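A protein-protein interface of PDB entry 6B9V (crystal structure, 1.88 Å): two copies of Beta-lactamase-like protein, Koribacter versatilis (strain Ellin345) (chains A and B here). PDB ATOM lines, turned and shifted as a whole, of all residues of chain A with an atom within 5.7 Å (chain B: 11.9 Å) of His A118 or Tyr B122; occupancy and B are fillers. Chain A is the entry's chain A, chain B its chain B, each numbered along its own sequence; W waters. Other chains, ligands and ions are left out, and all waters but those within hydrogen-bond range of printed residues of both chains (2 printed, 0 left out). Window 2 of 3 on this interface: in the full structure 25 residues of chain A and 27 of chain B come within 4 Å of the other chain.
His A118 touches just these residues of chain B: His B118 and Tyr B122. Tyr B122 touches just these residues of chain A: Arg A114 (3.8 Å), Val A115 (3.6 Å) and His A118 (3.6 Å). No residue of chain B comes within 4 Å of Lys A111. Val A115 touches two residues of chain B. No residue of chain B comes within 4 Å of Lys A121. Of the printed residues of chain B, Val A119 touches Val B119 (3.99 Å) and Ile B123 (3.7 Å). Of the printed residues of chain A, Val B119 touches Val A119 (3.99 Å). Lys B117 touches none of the printed residues of chain A. The nearest residue of chain B that does not touch His A118 is Val B119 (5.4 Å).
O of His A118 lies within hydrogen-bond range of NE2 of His B118, at 2.7 Å.
Water W2 lies within hydrogen-bond range of OH of Tyr B122 (2.5 Å) and NH1 of Arg A114 (3.5 Å). Water W1 lies within hydrogen-bond range of O of His B118 (2.6 Å), N of Tyr B122 (2.7 Å), NE2 of His A118 (2.7 Å), N of Lys B121 (3.4 Å) and O of Lys B117 (3.5 Å).
Tyr B122 touches Arg A114 (OH to NH1, 3.8 Å). Val A115 touches Tyr B122 (CG2 to CE2, 3.6 Å). CG1 of Val A115 touches CG2 of Ile B123, 3.6 Å away. His A118 touches Tyr B122. CG2 of Val A119 touches O of Val B119, at 3.99 Å. Val A119 touches Ile B123 (CG2 to CG2, 3.7 Å).
Hydrophobic or aromatic side chains of chain B within 4 Å of the printed part of chain A: His B118, Tyr B122 and Ile B123. Printed residues of chain A that touch a printed residue of chain B: Arg A114, Val A115, His A118 and Val A119.
His B118 touches its own counterpart, His A118. Val B119 touches its own counterpart, Val A119. Positions printed for both chains: 113, 114, 115, 116, 117, 118, 119, 120 and 121.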
ATOM      1  N   LYS A 111      20.695  17.392  17.978  1.00  0.00           N
ATOM      2  CA  LYS A 111      20.512  16.642  16.730  1.00  0.00           C
ATOM      3  C   LYS A 111      19.018  16.507  16.385  1.00  0.00           C
ATOM      4  O   LYS A 111      18.596  16.617  15.209  1.00  0.00           O
ATOM      5  CB  LYS A 111      21.169  15.262  16.816  1.00  0.00           C
ATOM      6  CG  LYS A 111      21.439  14.647  15.434  1.00  0.00           C
ATOM      7  CD  LYS A 111      21.882  13.189  15.521  1.00  0.00           C
ATOM      8  CE  LYS A 111      22.209  12.617  14.145  1.00  0.00           C
ATOM      9  NZ  LYS A 111      21.050  12.666  13.211  1.00  0.00           N
ATOM     10  N   GLU A 113      16.573  18.584  17.441  1.00  0.00           N
ATOM     11  CA  GLU A 113      16.164  19.924  17.053  1.00  0.00           C
ATOM     12  C   GLU A 113      16.483  20.179  15.580  1.00  0.00           C
ATOM     13  O   GLU A 113      15.638  20.677  14.848  1.00  0.00           O
ATOM     14  CB  GLU A 113      16.857  20.968  17.934  1.00  0.00           C
ATOM     15  CG  GLU A 113      16.613  22.392  17.487  1.00  0.00           C
ATOM     16  CD  GLU A 113      17.481  23.385  18.234  1.00  0.00           C
ATOM     17  OE1 GLU A 113      17.847  23.100  19.392  1.00  0.00           O
ATOM     18  OE2 GLU A 113      17.812  24.436  17.653  1.00  0.00           O
ATOM     19  N   ARG A 114      17.707  19.827  15.162  1.00  0.00           N
ATOM     20  CA  ARG A 114      18.156  20.012  13.773  1.00  0.00           C
ATOM     21  C   ARG A 114      17.204  19.318  12.779  1.00  0.00           C
ATOM     22  O   ARG A 114      16.774  19.912  11.751  1.00  0.00           O
ATOM     23  CB  ARG A 114      19.586  19.472  13.604  1.00  0.00           C
ATOM     24  CG  ARG A 114      20.394  20.061  12.454  1.00  0.00           C
ATOM     25  CD  ARG A 114      21.644  19.207  12.148  1.00  0.00           C
ATOM     26  NE  ARG A 114      22.372  18.810  13.356  1.00  0.00           N
ATOM     27  CZ  ARG A 114      23.339  17.897  13.393  1.00  0.00           C
ATOM     28  NH1 ARG A 114      23.718  17.272  12.287  1.00  0.00           N
ATOM     29  NH2 ARG A 114      23.937  17.607  14.545  1.00  0.00           N
ATOM     30  N   VAL A 115      16.875  18.064  13.086  1.00  0.00           N
ATOM     31  CA  VAL A 115      15.953  17.324  12.224  1.00  0.00           C
ATOM     32  C   VAL A 115      14.540  17.930  12.220  1.00  0.00           C
ATOM     33  O   VAL A 115      13.924  18.081  11.157  1.00  0.00           O
ATOM     34  CB  VAL A 115      15.875  15.831  12.641  1.00  0.00           C
ATOM     35  CG1 VAL A 115      14.823  15.098  11.816  1.00  0.00           C
ATOM     36  CG2 VAL A 115      17.250  15.167  12.507  1.00  0.00           C
ATOM     37  N   LEU A 116      14.019  18.270  13.394  1.00  0.00           N
ATOM     38  CA  LEU A 116      12.685  18.881  13.483  1.00  0.00           C
ATOM     39  C   LEU A 116      12.568  20.194  12.698  1.00  0.00           C
ATOM     40  O   LEU A 116      11.590  20.406  11.962  1.00  0.00           O
ATOM     41  CB  LEU A 116      12.293  19.144  14.943  1.00  0.00           C
ATOM     42  CG  LEU A 116      11.937  17.933  15.814  1.00  0.00           C
ATOM     43  CD1 LEU A 116      11.777  18.368  17.265  1.00  0.00           C
ATOM     44  CD2 LEU A 116      10.657  17.248  15.326  1.00  0.00           C
ATOM     45  N   LYS A 117      13.547  21.080  12.859  1.00  0.00           N
ATOM     46  CA  LYS A 117      13.495  22.364  12.168  1.00  0.00           C
ATOM     47  C   LYS A 117      13.636  22.172  10.665  1.00  0.00           C
ATOM     48  O   LYS A 117      13.061  22.937   9.880  1.00  0.00           O
ATOM     49  CB  LYS A 117      14.581  23.310  12.684  1.00  0.00           C
ATOM     50  CG  LYS A 117      14.323  23.781  14.107  1.00  0.00           C
ATOM     51  CD  LYS A 117      15.346  24.820  14.531  1.00  0.00           C
ATOM     52  CE  LYS A 117      14.922  25.506  15.819  1.00  0.00           C
ATOM     53  NZ  LYS A 117      15.939  26.490  16.279  1.00  0.00           N
ATOM     54  N   HIS A 118      14.399  21.159  10.261  1.00  0.00           N
ATOM     55  CA  HIS A 118      14.543  20.901   8.830  1.00  0.00           C
ATOM     56  C   HIS A 118      13.252  20.336   8.224  1.00  0.00           C
ATOM     57  O   HIS A 118      12.695  20.894   7.269  1.00  0.00           O
ATOM     58  CB  HIS A 118      15.716  19.946   8.584  1.00  0.00           C
ATOM     59  CG  HIS A 118      15.850  19.510   7.161  1.00  0.00           C
ATOM     60  ND1 HIS A 118      16.496  20.267   6.209  1.00  0.00           N
ATOM     61  CD2 HIS A 118      15.413  18.396   6.526  1.00  0.00           C
ATOM     62  CE1 HIS A 118      16.461  19.635   5.049  1.00  0.00           C
ATOM     63  NE2 HIS A 118      15.810  18.497   5.214  1.00  0.00           N
ATOM     64  N   VAL A 119      12.770  19.236   8.796  1.00  0.00           N
ATOM     65  CA  VAL A 119      11.587  18.549   8.300  1.00  0.00           C
ATOM     66  C   VAL A 119      10.347  19.429   8.395  1.00  0.00           C
ATOM     67  O   VAL A 119       9.530  19.458   7.477  1.00  0.00           O
ATOM     68  CB  VAL A 119      11.328  17.238   9.069  1.00  0.00           C
ATOM     69  CG1 VAL A 119       9.970  16.646   8.701  1.00  0.00           C
ATOM     70  CG2 VAL A 119      12.438  16.225   8.796  1.00  0.00           C
ATOM     71  N   PHE A 120      10.205  20.146   9.504  1.00  0.00           N
ATOM     72  CA  PHE A 120       9.011  20.950   9.728  1.00  0.00           C
ATOM     73  C   PHE A 120       9.343  22.423   9.623  1.00  0.00           C
ATOM     74  O   PHE A 120       8.852  23.237  10.403  1.00  0.00           O
ATOM     75  CB  PHE A 120       8.383  20.634  11.085  1.00  0.00           C
ATOM     76  CG  PHE A 120       7.763  19.264  11.151  1.00  0.00           C
ATOM     77  CD1 PHE A 120       6.579  18.995  10.472  1.00  0.00           C
ATOM     78  CD2 PHE A 120       8.370  18.246  11.867  1.00  0.00           C
ATOM     79  CE1 PHE A 120       6.006  17.736  10.515  1.00  0.00           C
ATOM     80  CE2 PHE A 120       7.802  16.983  11.915  1.00  0.00           C
ATOM     81  CZ  PHE A 120       6.617  16.728  11.242  1.00  0.00           C
ATOM     82  N   LYS A 121      10.171  22.752   8.637  1.00  0.00           N
ATOM     83  CA  LYS A 121      10.535  24.139   8.361  1.00  0.00           C
ATOM     84  C   LYS A 121       9.310  25.040   8.138  1.00  0.00           C
ATOM     85  O   LYS A 121       9.357  26.237   8.428  1.00  0.00           O
ATOM     86  CB  LYS A 121      11.461  24.199   7.148  1.00  0.00           C
ATOM     87  CG  LYS A 121      12.272  25.471   7.059  1.00  0.00           C
ATOM     88  CD  LYS A 121      12.958  25.578   5.711  1.00  0.00           C
ATOM     89  CE  LYS A 121      13.819  26.828   5.631  1.00  0.00           C
ATOM     90  NZ  LYS A 121      14.431  26.985   4.278  1.00  0.00           N
ATOM     91  N   GLY B  79       1.951  19.093  -2.638  1.00  0.00           N
ATOM     92  CA  GLY B  79       2.899  18.682  -1.620  1.00  0.00           C
ATOM     93  C   GLY B  79       2.569  19.026  -0.184  1.00  0.00           C
ATOM     94  O   GLY B  79       3.418  18.877   0.695  1.00  0.00           O
ATOM     95  N   ALA B  81       1.274  18.771   3.621  1.00  0.00           N
ATOM     96  CA  ALA B  81       1.492  17.678   4.571  1.00  0.00           C
ATOM     97  C   ALA B  81       0.340  16.668   4.644  1.00  0.00           C
ATOM     98  O   ALA B  81       0.594  15.480   4.756  1.00  0.00           O
ATOM     99  CB  ALA B  81       1.773  18.244   5.968  1.00  0.00           C
ATOM    100  N   ILE B  84       1.026  14.192   1.761  1.00  0.00           N
ATOM    101  CA  ILE B  84       2.319  13.536   1.525  1.00  0.00           C
ATOM    102  C   ILE B  84       2.933  12.806   2.727  1.00  0.00           C
ATOM    103  O   ILE B  84       3.794  11.953   2.535  1.00  0.00           O
ATOM    104  CB  ILE B  84       3.396  14.533   1.043  1.00  0.00           C
ATOM    105  CG1 ILE B  84       3.725  15.539   2.155  1.00  0.00           C
ATOM    106  CG2 ILE B  84       2.978  15.221  -0.238  1.00  0.00           C
ATOM    107  CD1 ILE B  84       5.040  16.268   1.931  1.00  0.00           C
ATOM    108  N   LEU B  85       2.519  13.129   3.948  1.00  0.00           N
ATOM    109  CA  LEU B  85       3.264  12.649   5.124  1.00  0.00           C
ATOM    110  C   LEU B  85       3.184  11.141   5.366  1.00  0.00           C
ATOM    111  O   LEU B  85       3.863  10.625   6.253  1.00  0.00           O
ATOM    112  CB  LEU B  85       2.819  13.379   6.389  1.00  0.00           C
ATOM    113  CG  LEU B  85       3.446  14.773   6.546  1.00  0.00           C
ATOM    114  CD1 LEU B  85       2.978  15.424   7.831  1.00  0.00           C
ATOM    115  CD2 LEU B  85       4.970  14.686   6.521  1.00  0.00           C
ATOM    116  N   LEU B  87       4.122   8.945   3.078  1.00  0.00           N
ATOM    117  CA  LEU B  87       5.057   8.298   2.154  1.00  0.00           C
ATOM    118  C   LEU B  87       6.007   7.383   2.919  1.00  0.00           C
ATOM    119  O   LEU B  87       6.384   6.323   2.434  1.00  0.00           O
ATOM    120  CB  LEU B  87       5.849   9.333   1.348  1.00  0.00           C
ATOM    121  CG  LEU B  87       6.813   8.755   0.304  1.00  0.00           C
ATOM    122  CD1 LEU B  87       6.068   7.851  -0.677  1.00  0.00           C
ATOM    123  CD2 LEU B  87       7.552   9.871  -0.447  1.00  0.00           C
ATOM    124  N   ASP B  88       6.366   7.784   4.133  1.00  0.00           N
ATOM    125  CA  ASP B  88       7.228   6.951   4.973  1.00  0.00           C
ATOM    126  C   ASP B  88       6.625   5.560   5.196  1.00  0.00           C
ATOM    127  O   ASP B  88       7.353   4.562   5.235  1.00  0.00           O
ATOM    128  CB  ASP B  88       7.488   7.650   6.312  1.00  0.00           C
ATOM    129  CG  ASP B  88       8.204   6.762   7.315  1.00  0.00           C
ATOM    130  OD1 ASP B  88       9.307   6.262   6.999  1.00  0.00           O
ATOM    131  OD2 ASP B  88       7.659   6.578   8.429  1.00  0.00           O
ATOM    132  N   ARG B  91       6.794   2.510   2.479  1.00  0.00           N
ATOM    133  CA  ARG B  91       8.049   1.748   2.317  1.00  0.00           C
ATOM    134  C   ARG B  91       7.919   0.212   2.321  1.00  0.00           C
ATOM    135  O   ARG B  91       8.442  -0.431   1.417  1.00  0.00           O
ATOM    136  CB  ARG B  91       9.064   2.181   3.385  1.00  0.00           C
ATOM    137  CG  ARG B  91       9.781   3.488   3.045  1.00  0.00           C
ATOM    138  CD  ARG B  91      10.200   4.233   4.302  1.00  0.00           C
ATOM    139  NE  ARG B  91      11.637   4.466   4.378  1.00  0.00           N
ATOM    140  CZ  ARG B  91      12.237   5.019   5.426  1.00  0.00           C
ATOM    141  NH1 ARG B  91      11.520   5.389   6.480  1.00  0.00           N
ATOM    142  NH2 ARG B  91      13.551   5.198   5.426  1.00  0.00           N
ATOM    143  N   GLU B 113       7.586  17.585  -6.240  1.00  0.00           N
ATOM    144  CA  GLU B 113       8.802  16.776  -6.150  1.00  0.00           C
ATOM    145  C   GLU B 113       9.814  17.415  -5.196  1.00  0.00           C
ATOM    146  O   GLU B 113      10.388  16.734  -4.343  1.00  0.00           O
ATOM    147  CB  GLU B 113       9.421  16.583  -7.539  1.00  0.00           C
ATOM    148  CG  GLU B 113      10.775  15.892  -7.511  1.00  0.00           C
ATOM    149  CD  GLU B 113      11.329  15.607  -8.901  1.00  0.00           C
ATOM    150  OE1 GLU B 113      10.712  16.019  -9.904  1.00  0.00           O
ATOM    151  OE2 GLU B 113      12.395  14.963  -8.986  1.00  0.00           O
ATOM    152  N   ARG B 114      10.014  18.728  -5.337  1.00  0.00           N
ATOM    153  CA  ARG B 114      10.940  19.459  -4.472  1.00  0.00           C
ATOM    154  C   ARG B 114      10.530  19.354  -3.010  1.00  0.00           C
ATOM    155  O   ARG B 114      11.374  19.122  -2.119  1.00  0.00           O
ATOM    156  CB  ARG B 114      11.038  20.936  -4.879  1.00  0.00           C
ATOM    157  CG  ARG B 114      11.810  21.133  -6.177  1.00  0.00           C
ATOM    158  CD  ARG B 114      12.224  22.582  -6.444  1.00  0.00           C
ATOM    159  NE  ARG B 114      11.307  23.583  -5.912  1.00  0.00           N
ATOM    160  CZ  ARG B 114      10.549  24.364  -6.674  1.00  0.00           C
ATOM    161  NH1 ARG B 114      10.583  24.230  -7.994  1.00  0.00           N
ATOM    162  NH2 ARG B 114       9.749  25.263  -6.118  1.00  0.00           N
ATOM    163  N   VAL B 115       9.232  19.524  -2.753  1.00  0.00           N
ATOM    164  CA  VAL B 115       8.748  19.358  -1.391  1.00  0.00           C
ATOM    165  C   VAL B 115       9.024  17.949  -0.849  1.00  0.00           C
ATOM    166  O   VAL B 115       9.564  17.797   0.252  1.00  0.00           O
ATOM    167  CB  VAL B 115       7.246  19.648  -1.289  1.00  0.00           C
ATOM    168  CG1 VAL B 115       6.732  19.246   0.083  1.00  0.00           C
ATOM    169  CG2 VAL B 115       6.992  21.106  -1.553  1.00  0.00           C
ATOM    170  N   LEU B 116       8.655  16.929  -1.625  1.00  0.00           N
ATOM    171  CA  LEU B 116       8.860  15.539  -1.207  1.00  0.00           C
ATOM    172  C   LEU B 116      10.324  15.286  -0.839  1.00  0.00           C
ATOM    173  O   LEU B 116      10.627  14.677   0.202  1.00  0.00           O
ATOM    174  CB  LEU B 116       8.413  14.577  -2.313  1.00  0.00           C
ATOM    175  CG  LEU B 116       6.893  14.490  -2.502  1.00  0.00           C
ATOM    176  CD1 LEU B 116       6.500  13.834  -3.828  1.00  0.00           C
ATOM    177  CD2 LEU B 116       6.261  13.755  -1.317  1.00  0.00           C
ATOM    178  N   LYS B 117      11.227  15.780  -1.685  1.00  0.00           N
ATOM    179  CA  LYS B 117      12.659  15.634  -1.430  1.00  0.00           C
ATOM    180  C   LYS B 117      13.105  16.354  -0.155  1.00  0.00           C
ATOM    181  O   LYS B 117      13.838  15.781   0.650  1.00  0.00           O
ATOM    182  CB  LYS B 117      13.470  16.129  -2.631  1.00  0.00           C
ATOM    183  CG  LYS B 117      13.284  15.268  -3.877  1.00  0.00           C
ATOM    184  CD  LYS B 117      14.230  15.652  -5.003  1.00  0.00           C
ATOM    185  CE  LYS B 117      13.995  14.772  -6.224  1.00  0.00           C
ATOM    186  NZ  LYS B 117      14.840  15.157  -7.394  1.00  0.00           N
ATOM    187  N   HIS B 118      12.670  17.599   0.050  1.00  0.00           N
ATOM    188  CA  HIS B 118      13.036  18.294   1.287  1.00  0.00           C
ATOM    189  C   HIS B 118      12.546  17.573   2.543  1.00  0.00           C
ATOM    190  O   HIS B 118      13.307  17.366   3.496  1.00  0.00           O
ATOM    191  CB  HIS B 118      12.493  19.722   1.310  1.00  0.00           C
ATOM    192  CG  HIS B 118      12.728  20.421   2.615  1.00  0.00           C
ATOM    193  ND1 HIS B 118      13.918  21.045   2.919  1.00  0.00           N
ATOM    194  CD2 HIS B 118      11.941  20.560   3.708  1.00  0.00           C
ATOM    195  CE1 HIS B 118      13.847  21.557   4.134  1.00  0.00           C
ATOM    196  NE2 HIS B 118      12.659  21.277   4.636  1.00  0.00           N
ATOM    197  N   VAL B 119      11.270  17.196   2.548  1.00  0.00           N
ATOM    198  CA  VAL B 119      10.681  16.583   3.731  1.00  0.00           C
ATOM    199  C   VAL B 119      11.266  15.205   4.025  1.00  0.00           C
ATOM    200  O   VAL B 119      11.444  14.842   5.191  1.00  0.00           O
ATOM    201  CB  VAL B 119       9.140  16.474   3.592  1.00  0.00           C
ATOM    202  CG1 VAL B 119       8.529  15.671   4.741  1.00  0.00           C
ATOM    203  CG2 VAL B 119       8.538  17.865   3.525  1.00  0.00           C
ATOM    204  N   PHE B 120      11.581  14.430   2.991  1.00  0.00           N
ATOM    205  CA  PHE B 120      11.992  13.054   3.261  1.00  0.00           C
ATOM    206  C   PHE B 120      13.463  12.676   2.999  1.00  0.00           C
ATOM    207  O   PHE B 120      13.897  11.619   3.440  1.00  0.00           O
ATOM    208  CB  PHE B 120      11.076  12.097   2.488  1.00  0.00           C
ATOM    209  CG  PHE B 120       9.692  11.984   3.090  1.00  0.00           C
ATOM    210  CD1 PHE B 120       9.517  11.427   4.351  1.00  0.00           C
ATOM    211  CD2 PHE B 120       8.582  12.466   2.413  1.00  0.00           C
ATOM    212  CE1 PHE B 120       8.256  11.328   4.927  1.00  0.00           C
ATOM    213  CE2 PHE B 120       7.312  12.375   2.975  1.00  0.00           C
ATOM    214  CZ  PHE B 120       7.148  11.805   4.232  1.00  0.00           C
ATOM    215  N   LYS B 121      14.255  13.509   2.333  1.00  0.00           N
ATOM    216  CA  LYS B 121      15.613  13.050   2.016  1.00  0.00           C
ATOM    217  C   LYS B 121      16.632  13.310   3.155  1.00  0.00           C
ATOM    218  O   LYS B 121      17.830  13.068   3.005  1.00  0.00           O
ATOM    219  CB  LYS B 121      16.095  13.679   0.706  1.00  0.00           C
ATOM    220  CG  LYS B 121      17.434  13.145   0.204  1.00  0.00           C
ATOM    221  CD  LYS B 121      17.929  13.855  -1.025  1.00  0.00           C
ATOM    222  CE  LYS B 121      19.442  13.743  -1.115  1.00  0.00           C
ATOM    223  NZ  LYS B 121      20.100  13.753   0.232  1.00  0.00           N
ATOM    224  N   TYR B 122      16.179  13.783   4.305  1.00  0.00           N
ATOM    225  CA  TYR B 122      17.081  13.802   5.456  1.00  0.00           C
ATOM    226  C   TYR B 122      16.765  12.587   6.321  1.00  0.00           C
ATOM    227  O   TYR B 122      17.664  11.843   6.711  1.00  0.00           O
ATOM    228  CB  TYR B 122      16.963  15.104   6.271  1.00  0.00           C
ATOM    229  CG  TYR B 122      18.011  15.246   7.377  1.00  0.00           C
ATOM    230  CD1 TYR B 122      19.190  14.500   7.350  1.00  0.00           C
ATOM    231  CD2 TYR B 122      17.814  16.113   8.449  1.00  0.00           C
ATOM    232  CE1 TYR B 122      20.144  14.616   8.357  1.00  0.00           C
ATOM    233  CE2 TYR B 122      18.760  16.235   9.468  1.00  0.00           C
ATOM    234  CZ  TYR B 122      19.921  15.483   9.414  1.00  0.00           C
ATOM    235  OH  TYR B 122      20.863  15.599  10.414  1.00  0.00           O
ATOM    236  N   ILE B 123      15.479  12.374   6.581  1.00  0.00           N
ATOM    237  CA  ILE B 123      15.034  11.317   7.488  1.00  0.00           C
ATOM    238  C   ILE B 123      14.781   9.968   6.820  1.00  0.00           C
ATOM    239  O   ILE B 123      14.090   9.122   7.386  1.00  0.00           O
ATOM    240  CB  ILE B 123      13.737  11.718   8.199  1.00  0.00           C
ATOM    241  CG1 ILE B 123      12.692  12.138   7.172  1.00  0.00           C
ATOM    242  CG2 ILE B 123      13.987  12.850   9.171  1.00  0.00           C
ATOM    243  CD1 ILE B 123      11.290  12.175   7.723  1.00  0.00           C
HETATM  244  O   HOH W   1      15.742  16.353   3.521  1.00  0.00           O
HETATM  245  O   HOH W   2      22.948  14.286  10.691  1.00  0.00           O
